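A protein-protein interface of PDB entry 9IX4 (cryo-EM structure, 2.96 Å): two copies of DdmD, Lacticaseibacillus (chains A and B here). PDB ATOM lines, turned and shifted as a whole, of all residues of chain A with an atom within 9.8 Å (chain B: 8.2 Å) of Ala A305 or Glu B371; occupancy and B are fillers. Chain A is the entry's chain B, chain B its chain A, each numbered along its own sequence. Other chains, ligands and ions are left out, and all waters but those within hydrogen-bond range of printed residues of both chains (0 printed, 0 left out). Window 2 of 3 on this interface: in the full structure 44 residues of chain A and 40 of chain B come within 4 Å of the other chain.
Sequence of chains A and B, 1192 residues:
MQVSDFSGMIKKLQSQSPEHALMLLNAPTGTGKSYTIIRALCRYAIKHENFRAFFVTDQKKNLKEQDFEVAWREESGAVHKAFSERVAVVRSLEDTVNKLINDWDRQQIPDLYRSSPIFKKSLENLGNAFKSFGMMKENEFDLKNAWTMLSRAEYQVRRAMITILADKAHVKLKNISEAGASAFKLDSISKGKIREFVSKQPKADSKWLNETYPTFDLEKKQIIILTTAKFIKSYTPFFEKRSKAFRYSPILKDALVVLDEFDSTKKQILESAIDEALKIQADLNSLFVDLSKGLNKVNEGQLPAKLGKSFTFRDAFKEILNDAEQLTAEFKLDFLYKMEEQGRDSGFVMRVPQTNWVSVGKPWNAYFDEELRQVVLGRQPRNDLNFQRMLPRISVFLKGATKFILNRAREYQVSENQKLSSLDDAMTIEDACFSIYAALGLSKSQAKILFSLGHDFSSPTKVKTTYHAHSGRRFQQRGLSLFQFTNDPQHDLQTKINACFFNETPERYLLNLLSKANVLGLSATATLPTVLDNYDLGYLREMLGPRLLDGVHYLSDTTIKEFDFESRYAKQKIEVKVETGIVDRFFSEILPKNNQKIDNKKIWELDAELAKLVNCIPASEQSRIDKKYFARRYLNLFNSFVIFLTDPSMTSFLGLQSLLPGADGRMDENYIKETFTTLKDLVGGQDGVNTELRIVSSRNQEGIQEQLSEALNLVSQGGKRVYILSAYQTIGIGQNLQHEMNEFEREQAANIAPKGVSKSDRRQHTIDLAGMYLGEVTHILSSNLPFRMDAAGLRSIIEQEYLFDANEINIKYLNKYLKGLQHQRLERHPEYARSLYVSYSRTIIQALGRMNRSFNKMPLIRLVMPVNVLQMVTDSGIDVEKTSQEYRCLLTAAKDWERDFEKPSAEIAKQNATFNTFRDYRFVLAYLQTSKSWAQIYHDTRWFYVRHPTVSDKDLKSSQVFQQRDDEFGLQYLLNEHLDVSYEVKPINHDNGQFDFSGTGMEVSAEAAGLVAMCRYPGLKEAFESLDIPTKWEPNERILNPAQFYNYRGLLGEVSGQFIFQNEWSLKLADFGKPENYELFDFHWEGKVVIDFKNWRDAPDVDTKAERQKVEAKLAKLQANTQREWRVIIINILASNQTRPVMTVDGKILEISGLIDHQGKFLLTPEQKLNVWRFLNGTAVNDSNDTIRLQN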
ATOM      1  N   VAL A 298      16.123 -14.363 -11.893  1.00  0.00           N
ATOM      2  CA  VAL A 298      16.742 -15.605 -11.442  1.00  0.00           C
ATOM      3  C   VAL A 298      16.016 -16.802 -12.034  1.00  0.00           C
ATOM      4  O   VAL A 298      16.639 -17.798 -12.417  1.00  0.00           O
ATOM      5  CB  VAL A 298      16.765 -15.679  -9.908  1.00  0.00           C
ATOM      6  CG1 VAL A 298      17.513 -16.912  -9.473  1.00  0.00           C
ATOM      7  CG2 VAL A 298      17.403 -14.452  -9.327  1.00  0.00           C
ATOM      8  N   GLY A 301      16.851 -17.910 -15.663  1.00  0.00           N
ATOM      9  CA  GLY A 301      18.243 -18.245 -15.907  1.00  0.00           C
ATOM     10  C   GLY A 301      19.052 -17.120 -16.509  1.00  0.00           C
ATOM     11  O   GLY A 301      19.865 -17.358 -17.410  1.00  0.00           O
ATOM     12  N   GLN A 302      18.846 -15.894 -16.037  1.00  0.00           N
ATOM     13  CA  GLN A 302      19.588 -14.740 -16.520  1.00  0.00           C
ATOM     14  C   GLN A 302      20.631 -14.259 -15.527  1.00  0.00           C
ATOM     15  O   GLN A 302      21.092 -13.121 -15.632  1.00  0.00           O
ATOM     16  CB  GLN A 302      18.629 -13.608 -16.867  1.00  0.00           C
ATOM     17  CG  GLN A 302      17.843 -13.882 -18.120  1.00  0.00           C
ATOM     18  CD  GLN A 302      16.892 -12.772 -18.462  1.00  0.00           C
ATOM     19  OE1 GLN A 302      16.784 -11.788 -17.737  1.00  0.00           O
ATOM     20  NE2 GLN A 302      16.186 -12.925 -19.570  1.00  0.00           N
ATOM     21  N   LEU A 303      21.007 -15.088 -14.571  1.00  0.00           N
ATOM     22  CA  LEU A 303      22.082 -14.796 -13.644  1.00  0.00           C
ATOM     23  C   LEU A 303      23.107 -15.916 -13.708  1.00  0.00           C
ATOM     24  O   LEU A 303      22.787 -17.030 -14.138  1.00  0.00           O
ATOM     25  CB  LEU A 303      21.560 -14.645 -12.210  1.00  0.00           C
ATOM     26  CG  LEU A 303      20.759 -13.376 -11.944  1.00  0.00           C
ATOM     27  CD1 LEU A 303      20.464 -13.279 -10.479  1.00  0.00           C
ATOM     28  CD2 LEU A 303      21.510 -12.154 -12.414  1.00  0.00           C
ATOM     29  N   PRO A 304      24.348 -15.660 -13.297  1.00  0.00           N
ATOM     30  CA  PRO A 304      25.387 -16.682 -13.430  1.00  0.00           C
ATOM     31  C   PRO A 304      24.982 -17.974 -12.743  1.00  0.00           C
ATOM     32  O   PRO A 304      24.258 -17.974 -11.747  1.00  0.00           O
ATOM     33  CB  PRO A 304      26.606 -16.047 -12.754  1.00  0.00           C
ATOM     34  CG  PRO A 304      26.095 -14.849 -12.044  1.00  0.00           C
ATOM     35  CD  PRO A 304      24.901 -14.397 -12.790  1.00  0.00           C
ATOM     36  N   ALA A 305      25.445 -19.090 -13.309  1.00  0.00           N
ATOM     37  CA  ALA A 305      24.997 -20.396 -12.844  1.00  0.00           C
ATOM     38  C   ALA A 305      25.317 -20.614 -11.374  1.00  0.00           C
ATOM     39  O   ALA A 305      24.620 -21.382 -10.702  1.00  0.00           O
ATOM     40  CB  ALA A 305      25.630 -21.495 -13.693  1.00  0.00           C
ATOM     41  N   LYS A 306      26.326 -19.910 -10.853  1.00  0.00           N
ATOM     42  CA  LYS A 306      26.787 -20.109  -9.485  1.00  0.00           C
ATOM     43  C   LYS A 306      25.643 -20.011  -8.483  1.00  0.00           C
ATOM     44  O   LYS A 306      25.448 -20.905  -7.654  1.00  0.00           O
ATOM     45  CB  LYS A 306      27.869 -19.083  -9.156  1.00  0.00           C
ATOM     46  CG  LYS A 306      29.266 -19.520  -9.511  1.00  0.00           C
ATOM     47  CD  LYS A 306      30.109 -18.335  -9.938  1.00  0.00           C
ATOM     48  CE  LYS A 306      30.155 -17.277  -8.860  1.00  0.00           C
ATOM     49  NZ  LYS A 306      31.099 -16.186  -9.207  1.00  0.00           N
ATOM     50  N   LEU A 307      24.866 -18.932  -8.547  1.00  0.00           N
ATOM     51  CA  LEU A 307      23.721 -18.811  -7.658  1.00  0.00           C
ATOM     52  C   LEU A 307      22.423 -19.250  -8.312  1.00  0.00           C
ATOM     53  O   LEU A 307      21.494 -19.657  -7.603  1.00  0.00           O
ATOM     54  CB  LEU A 307      23.572 -17.372  -7.157  1.00  0.00           C
ATOM     55  CG  LEU A 307      23.183 -16.283  -8.151  1.00  0.00           C
ATOM     56  CD1 LEU A 307      21.682 -16.084  -8.200  1.00  0.00           C
ATOM     57  CD2 LEU A 307      23.829 -15.007  -7.752  1.00  0.00           C
ATOM     58  N   GLY A 308      22.338 -19.176  -9.638  1.00  0.00           N
ATOM     59  CA  GLY A 308      21.119 -19.580 -10.308  1.00  0.00           C
ATOM     60  C   GLY A 308      20.783 -21.036 -10.072  1.00  0.00           C
ATOM     61  O   GLY A 308      19.624 -21.384  -9.839  1.00  0.00           O
ATOM     62  N   LYS A 309      21.787 -21.911 -10.123  1.00  0.00           N
ATOM     63  CA  LYS A 309      21.505 -23.324  -9.916  1.00  0.00           C
ATOM     64  C   LYS A 309      21.191 -23.649  -8.466  1.00  0.00           C
ATOM     65  O   LYS A 309      20.669 -24.735  -8.195  1.00  0.00           O
ATOM     66  CB  LYS A 309      22.675 -24.176 -10.407  1.00  0.00           C
ATOM     67  CG  LYS A 309      23.844 -24.263  -9.448  1.00  0.00           C
ATOM     68  CD  LYS A 309      24.982 -25.053 -10.069  1.00  0.00           C
ATOM     69  CE  LYS A 309      25.376 -24.472 -11.419  1.00  0.00           C
ATOM     70  NZ  LYS A 309      26.302 -25.357 -12.173  1.00  0.00           N
ATOM     71  N   SER A 310      21.487 -22.745  -7.536  1.00  0.00           N
ATOM     72  CA  SER A 310      21.128 -22.941  -6.139  1.00  0.00           C
ATOM     73  C   SER A 310      19.767 -22.358  -5.803  1.00  0.00           C
ATOM     74  O   SER A 310      19.108 -22.840  -4.879  1.00  0.00           O
ATOM     75  CB  SER A 310      22.182 -22.318  -5.226  1.00  0.00           C
ATOM     76  OG  SER A 310      22.043 -20.912  -5.184  1.00  0.00           O
ATOM     77  N   PHE A 311      19.338 -21.325  -6.525  1.00  0.00           N
ATOM     78  CA  PHE A 311      18.006 -20.773  -6.309  1.00  0.00           C
ATOM     79  C   PHE A 311      16.927 -21.724  -6.807  1.00  0.00           C
ATOM     80  O   PHE A 311      15.940 -21.981  -6.111  1.00  0.00           O
ATOM     81  CB  PHE A 311      17.875 -19.430  -7.021  1.00  0.00           C
ATOM     82  CG  PHE A 311      18.264 -18.250  -6.191  1.00  0.00           C
ATOM     83  CD1 PHE A 311      19.573 -18.057  -5.804  1.00  0.00           C
ATOM     84  CD2 PHE A 311      17.320 -17.313  -5.821  1.00  0.00           C
ATOM     85  CE1 PHE A 311      19.930 -16.965  -5.053  1.00  0.00           C
ATOM     86  CE2 PHE A 311      17.672 -16.219  -5.071  1.00  0.00           C
ATOM     87  CZ  PHE A 311      18.978 -16.046  -4.685  1.00  0.00           C
ATOM     88  N   THR A 312      17.101 -22.260  -8.014  1.00  0.00           N
ATOM     89  CA  THR A 312      15.986 -22.809  -8.775  1.00  0.00           C
ATOM     90  C   THR A 312      15.546 -24.197  -8.335  1.00  0.00           C
ATOM     91  O   THR A 312      14.409 -24.583  -8.628  1.00  0.00           O
ATOM     92  CB  THR A 312      16.343 -22.854 -10.257  1.00  0.00           C
ATOM     93  OG1 THR A 312      17.601 -23.513 -10.422  1.00  0.00           O
ATOM     94  CG2 THR A 312      16.438 -21.451 -10.820  1.00  0.00           C
ATOM     95  N   PHE A 313      16.389 -24.961  -7.654  1.00  0.00           N
ATOM     96  CA  PHE A 313      16.032 -26.340  -7.355  1.00  0.00           C
ATOM     97  C   PHE A 313      15.208 -26.480  -6.083  1.00  0.00           C
ATOM     98  O   PHE A 313      14.853 -27.603  -5.715  1.00  0.00           O
ATOM     99  CB  PHE A 313      17.287 -27.211  -7.258  1.00  0.00           C
ATOM    100  CG  PHE A 313      17.990 -27.125  -5.942  1.00  0.00           C
ATOM    101  CD1 PHE A 313      18.880 -26.104  -5.688  1.00  0.00           C
ATOM    102  CD2 PHE A 313      17.787 -28.090  -4.972  1.00  0.00           C
ATOM    103  CE1 PHE A 313      19.536 -26.032  -4.480  1.00  0.00           C
ATOM    104  CE2 PHE A 313      18.437 -28.023  -3.765  1.00  0.00           C
ATOM    105  CZ  PHE A 313      19.315 -26.993  -3.517  1.00  0.00           C
ATOM    106  N   TYR A 412      26.394 -19.495  -0.963  1.00  0.00           N
ATOM    107  CA  TYR A 412      27.311 -18.911  -1.935  1.00  0.00           C
ATOM    108  C   TYR A 412      28.629 -18.518  -1.288  1.00  0.00           C
ATOM    109  O   TYR A 412      29.699 -18.754  -1.855  1.00  0.00           O
ATOM    110  CB  TYR A 412      26.646 -17.707  -2.597  1.00  0.00           C
ATOM    111  CG  TYR A 412      27.572 -16.829  -3.395  1.00  0.00           C
ATOM    112  CD1 TYR A 412      28.024 -17.219  -4.642  1.00  0.00           C
ATOM    113  CD2 TYR A 412      27.970 -15.596  -2.914  1.00  0.00           C
ATOM    114  CE1 TYR A 412      28.860 -16.415  -5.375  1.00  0.00           C
ATOM    115  CE2 TYR A 412      28.805 -14.786  -3.639  1.00  0.00           C
ATOM    116  CZ  TYR A 412      29.248 -15.199  -4.868  1.00  0.00           C
ATOM    117  OH  TYR A 412      30.085 -14.391  -5.595  1.00  0.00           O
ATOM    118  N   SER A 415      30.660 -21.677  -0.538  1.00  0.00           N
ATOM    119  CA  SER A 415      31.253 -22.238  -1.748  1.00  0.00           C
ATOM    120  C   SER A 415      32.409 -21.382  -2.247  1.00  0.00           C
ATOM    121  O   SER A 415      33.440 -21.909  -2.674  1.00  0.00           O
ATOM    122  CB  SER A 415      30.198 -22.386  -2.840  1.00  0.00           C
ATOM    123  OG  SER A 415      29.928 -21.140  -3.449  1.00  0.00           O
ATOM    124  N   GLU A 416      32.258 -20.057  -2.202  1.00  0.00           N
ATOM    125  CA  GLU A 416      33.298 -19.180  -2.724  1.00  0.00           C
ATOM    126  C   GLU A 416      34.549 -19.205  -1.863  1.00  0.00           C
ATOM    127  O   GLU A 416      35.659 -19.099  -2.390  1.00  0.00           O
ATOM    128  CB  GLU A 416      32.778 -17.751  -2.837  1.00  0.00           C
ATOM    129  CG  GLU A 416      31.868 -17.528  -4.016  1.00  0.00           C
ATOM    130  CD  GLU A 416      32.524 -17.879  -5.330  1.00  0.00           C
ATOM    131  OE1 GLU A 416      33.411 -17.125  -5.774  1.00  0.00           O
ATOM    132  OE2 GLU A 416      32.147 -18.911  -5.923  1.00  0.00           O
ATOM    133  N   LYS A 419      37.291 -21.677  -2.927  1.00  0.00           N
ATOM    134  CA  LYS A 419      38.195 -21.335  -4.020  1.00  0.00           C
ATOM    135  C   LYS A 419      39.409 -20.572  -3.515  1.00  0.00           C
ATOM    136  O   LYS A 419      40.526 -20.775  -4.004  1.00  0.00           O
ATOM    137  CB  LYS A 419      37.457 -20.515  -5.076  1.00  0.00           C
ATOM    138  CG  LYS A 419      36.677 -21.338  -6.081  1.00  0.00           C
ATOM    139  CD  LYS A 419      35.267 -21.608  -5.599  1.00  0.00           C
ATOM    140  CE  LYS A 419      34.431 -22.255  -6.686  1.00  0.00           C
ATOM    141  NZ  LYS A 419      33.164 -22.814  -6.146  1.00  0.00           N
ATOM    142  N   ILE A 436      24.604 -10.727  -3.791  1.00  0.00           N
ATOM    143  CA  ILE A 436      23.386 -11.341  -4.311  1.00  0.00           C
ATOM    144  C   ILE A 436      22.362 -10.270  -4.659  1.00  0.00           C
ATOM    145  O   ILE A 436      21.735 -10.310  -5.722  1.00  0.00           O
ATOM    146  CB  ILE A 436      22.818 -12.350  -3.299  1.00  0.00           C
ATOM    147  CG1 ILE A 436      23.783 -13.514  -3.095  1.00  0.00           C
ATOM    148  CG2 ILE A 436      21.486 -12.879  -3.777  1.00  0.00           C
ATOM    149  CD1 ILE A 436      23.790 -14.504  -4.211  1.00  0.00           C
ATOM    150  N   ALA A 439      23.407  -8.388  -7.780  1.00  0.00           N
ATOM    151  CA  ALA A 439      23.203  -9.198  -8.974  1.00  0.00           C
ATOM    152  C   ALA A 439      21.738  -9.252  -9.365  1.00  0.00           C
ATOM    153  O   ALA A 439      21.417  -9.376 -10.551  1.00  0.00           O
ATOM    154  CB  ALA A 439      23.740 -10.609  -8.755  1.00  0.00           C
ATOM    155  N   PHE B 335      22.327 -10.041 -19.117  1.00  0.00           N
ATOM    156  CA  PHE B 335      23.256 -10.803 -18.302  1.00  0.00           C
ATOM    157  C   PHE B 335      24.313  -9.888 -17.698  1.00  0.00           C
ATOM    158  O   PHE B 335      24.497  -8.743 -18.112  1.00  0.00           O
ATOM    159  CB  PHE B 335      23.911 -11.903 -19.136  1.00  0.00           C
ATOM    160  CG  PHE B 335      22.939 -12.898 -19.688  1.00  0.00           C
ATOM    161  CD1 PHE B 335      22.277 -12.654 -20.872  1.00  0.00           C
ATOM    162  CD2 PHE B 335      22.692 -14.078 -19.025  1.00  0.00           C
ATOM    163  CE1 PHE B 335      21.384 -13.565 -21.376  1.00  0.00           C
ATOM    164  CE2 PHE B 335      21.802 -14.992 -19.528  1.00  0.00           C
ATOM    165  CZ  PHE B 335      21.146 -14.734 -20.704  1.00  0.00           C
ATOM    166  N   PHE B 368      29.947 -13.934 -24.604  1.00  0.00           N
ATOM    167  CA  PHE B 368      28.975 -14.595 -23.745  1.00  0.00           C
ATOM    168  C   PHE B 368      29.435 -16.017 -23.452  1.00  0.00           C
ATOM    169  O   PHE B 368      29.582 -16.829 -24.370  1.00  0.00           O
ATOM    170  CB  PHE B 368      27.595 -14.610 -24.395  1.00  0.00           C
ATOM    171  CG  PHE B 368      26.541 -15.242 -23.543  1.00  0.00           C
ATOM    172  CD1 PHE B 368      26.151 -14.653 -22.359  1.00  0.00           C
ATOM    173  CD2 PHE B 368      25.943 -16.426 -23.920  1.00  0.00           C
ATOM    174  CE1 PHE B 368      25.190 -15.232 -21.568  1.00  0.00           C
ATOM    175  CE2 PHE B 368      24.977 -17.006 -23.130  1.00  0.00           C
ATOM    176  CZ  PHE B 368      24.601 -16.407 -21.955  1.00  0.00           C
ATOM    177  N   ASP B 369      29.667 -16.312 -22.178  1.00  0.00           N
ATOM    178  CA  ASP B 369      29.966 -17.663 -21.728  1.00  0.00           C
ATOM    179  C   ASP B 369      28.656 -18.333 -21.341  1.00  0.00           C
ATOM    180  O   ASP B 369      28.007 -17.930 -20.368  1.00  0.00           O
ATOM    181  CB  ASP B 369      30.939 -17.641 -20.554  1.00  0.00           C
ATOM    182  CG  ASP B 369      31.621 -18.971 -20.342  1.00  0.00           C
ATOM    183  OD1 ASP B 369      30.927 -20.007 -20.391  1.00  0.00           O
ATOM    184  OD2 ASP B 369      32.849 -18.985 -20.124  1.00  0.00           O
ATOM    185  N   GLU B 370      28.268 -19.354 -22.108  1.00  0.00           N
ATOM    186  CA  GLU B 370      26.989 -20.017 -21.882  1.00  0.00           C
ATOM    187  C   GLU B 370      27.039 -20.921 -20.659  1.00  0.00           C
ATOM    188  O   GLU B 370      26.060 -21.015 -19.911  1.00  0.00           O
ATOM    189  CB  GLU B 370      26.593 -20.818 -23.117  1.00  0.00           C
ATOM    190  CG  GLU B 370      26.379 -19.969 -24.348  1.00  0.00           C
ATOM    191  CD  GLU B 370      26.184 -20.796 -25.595  1.00  0.00           C
ATOM    192  OE1 GLU B 370      26.395 -22.024 -25.531  1.00  0.00           O
ATOM    193  OE2 GLU B 370      25.818 -20.220 -26.638  1.00  0.00           O
ATOM    194  N   GLU B 371      28.160 -21.611 -20.452  1.00  0.00           N
ATOM    195  CA  GLU B 371      28.275 -22.476 -19.285  1.00  0.00           C
ATOM    196  C   GLU B 371      28.201 -21.671 -17.997  1.00  0.00           C
ATOM    197  O   GLU B 371      27.570 -22.099 -17.025  1.00  0.00           O
ATOM    198  CB  GLU B 371      29.573 -23.277 -19.348  1.00  0.00           C
ATOM    199  CG  GLU B 371      29.639 -24.236 -20.520  1.00  0.00           C
ATOM    200  CD  GLU B 371      28.368 -25.051 -20.673  1.00  0.00           C
ATOM    201  OE1 GLU B 371      27.925 -25.659 -19.676  1.00  0.00           O
ATOM    202  OE2 GLU B 371      27.811 -25.081 -21.789  1.00  0.00           O
ATOM    203  N   LEU B 372      28.839 -20.505 -17.970  1.00  0.00           N
ATOM    204  CA  LEU B 372      28.770 -19.638 -16.805  1.00  0.00           C
ATOM    205  C   LEU B 372      27.507 -18.796 -16.772  1.00  0.00           C
ATOM    206  O   LEU B 372      27.228 -18.178 -15.739  1.00  0.00           O
ATOM    207  CB  LEU B 372      29.990 -18.720 -16.763  1.00  0.00           C
ATOM    208  CG  LEU B 372      31.335 -19.391 -16.506  1.00  0.00           C
ATOM    209  CD1 LEU B 372      32.409 -18.343 -16.309  1.00  0.00           C
ATOM    210  CD2 LEU B 372      31.246 -20.299 -15.301  1.00  0.00           C
ATOM    211  N   ARG B 373      26.741 -18.764 -17.861  1.00  0.00           N
ATOM    212  CA  ARG B 373      25.584 -17.880 -17.993  1.00  0.00           C
ATOM    213  C   ARG B 373      25.983 -16.438 -17.701  1.00  0.00           C
ATOM    214  O   ARG B 373      25.309 -15.713 -16.970  1.00  0.00           O
ATOM    215  CB  ARG B 373      24.439 -18.326 -17.086  1.00  0.00           C
ATOM    216  CG  ARG B 373      23.944 -19.727 -17.361  1.00  0.00           C
ATOM    217  CD  ARG B 373      23.248 -19.832 -18.698  1.00  0.00           C
ATOM    218  NE  ARG B 373      22.006 -19.073 -18.739  1.00  0.00           N
ATOM    219  CZ  ARG B 373      21.350 -18.781 -19.852  1.00  0.00           C
ATOM    220  NH1 ARG B 373      21.793 -19.171 -21.036  1.00  0.00           N
ATOM    221  NH2 ARG B 373      20.221 -18.085 -19.778  1.00  0.00           N
ATOM    222  N   GLN B 374      27.106 -16.024 -18.277  1.00  0.00           N
ATOM    223  CA  GLN B 374      27.687 -14.735 -17.940  1.00  0.00           C
ATOM    224  C   GLN B 374      28.246 -14.097 -19.199  1.00  0.00           C
ATOM    225  O   GLN B 374      28.264 -14.706 -20.266  1.00  0.00           O
ATOM    226  CB  GLN B 374      28.789 -14.888 -16.895  1.00  0.00           C
ATOM    227  CG  GLN B 374      28.914 -13.745 -15.931  1.00  0.00           C
ATOM    228  CD  GLN B 374      29.968 -14.011 -14.887  1.00  0.00           C
ATOM    229  OE1 GLN B 374      31.030 -14.552 -15.187  1.00  0.00           O
ATOM    230  NE2 GLN B 374      29.678 -13.645 -13.646  1.00  0.00           N
ATOM    231  N   LEU B 493      29.694 -10.373  -8.039  1.00  0.00           N
ATOM    232  CA  LEU B 493      29.251 -11.150  -9.187  1.00  0.00           C
ATOM    233  C   LEU B 493      29.319 -10.397 -10.505  1.00  0.00           C
ATOM    234  O   LEU B 493      29.110 -11.011 -11.555  1.00  0.00           O
ATOM    235  CB  LEU B 493      27.823 -11.621  -8.949  1.00  0.00           C
ATOM    236  CG  LEU B 493      27.735 -12.638  -7.823  1.00  0.00           C
ATOM    237  CD1 LEU B 493      26.323 -12.756  -7.377  1.00  0.00           C
ATOM    238  CD2 LEU B 493      28.233 -13.971  -8.320  1.00  0.00           C
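Among the printed residues, merely in contact across the chains: Gly A301 with Phe B335 (3.7 Å), Gln A302 with Phe B335 (3.7 Å), Leu A303 with Arg B373 (3.6 Å), Pro A304 with Leu B372 (3.3 Å), Pro A304 with Arg B373 (3.7 Å), Ala A305 with Glu B371 (3.9 Å), Ala A305 with Arg B373 (3.98 Å), Lys A306 with Leu B493 (3.7 Å), Leu A307 with Leu B493 (3.4 Å), Tyr A412 with Leu B493 (3.3 Å) and Ala A439 with Leu B493 (3.6 Å).
Val A298 touches none of the printed residues of chain B. Of the printed residues of chain B, Ala A305 touches Glu B371, Leu B372 and Arg B373. Of the printed residues of chain B, Lys A306 touches Leu B493. Of the printed residues of chain A, Leu B493 touches Lys A306, Leu A307, Tyr A412 and Ala A439. The nearest printed residue of chain B that does not touch Gln A302 is Arg B373 (4.5 Å).
Along chain B the printed residues that touch a printed residue of chain A span positions 335 to 493. Of the 20 printed residues of chain A, 9 touch a printed residue of chain B. Printed residues of chain A that touch a printed residue of chain B: Gly A301, Gln A302, Leu A303, Pro A304, Ala A305, Lys A306, Leu A307, Tyr A412 and Ala A439. Hydrophobic or aromatic side chains of chain A that line the printed part of chain B: Pro A304, Ala A305, Leu A307, Tyr A412 and Ala A439. Along chain A the printed residues that touch a printed residue of chain B span positions 301 to 439. Among the printed residues, no Asp or Glu carboxylate lies within 4 Å of a Lys or Arg side-chain nitrogen of the other chain.
No position is printed for both chains. Of the 13 pairs that touch across the chains among the printed residues, none has its exchanged pair printed and touching as well.
The backbone carbonyl oxygen (O) of Leu B372 is in hydrogen-bond range of the backbone NH (N) of Ala A305, at 3.1 Å. The backbone carbonyl oxygen of Gly A301 is in hydrogen-bond range of the guanidinium group of Arg B373 (2.5 Å).
OD1 of Asp B369 is in hydrogen-bond range of N of Glu B371, at 3.2 Å. The side-chain carboxylate (OD1) of Asp B369 is in hydrogen-bond range of the backbone NH (N) of Leu B372, 3.2 Å away. The backbone carbonyl oxygen (O) of Leu B493 is in hydrogen-bond range of the side-chain amide nitrogen (NE2) of Gln B374 (3.4 Å). The backbone carbonyl oxygen (O) of Leu A307 sits at hydrogen-bond distance from the side-chain hydroxyl (OG) of Ser A310 (2.8 Å). O of Tyr A412 sits at hydrogen-bond distance from OG of Ser A415 (2.9 Å).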
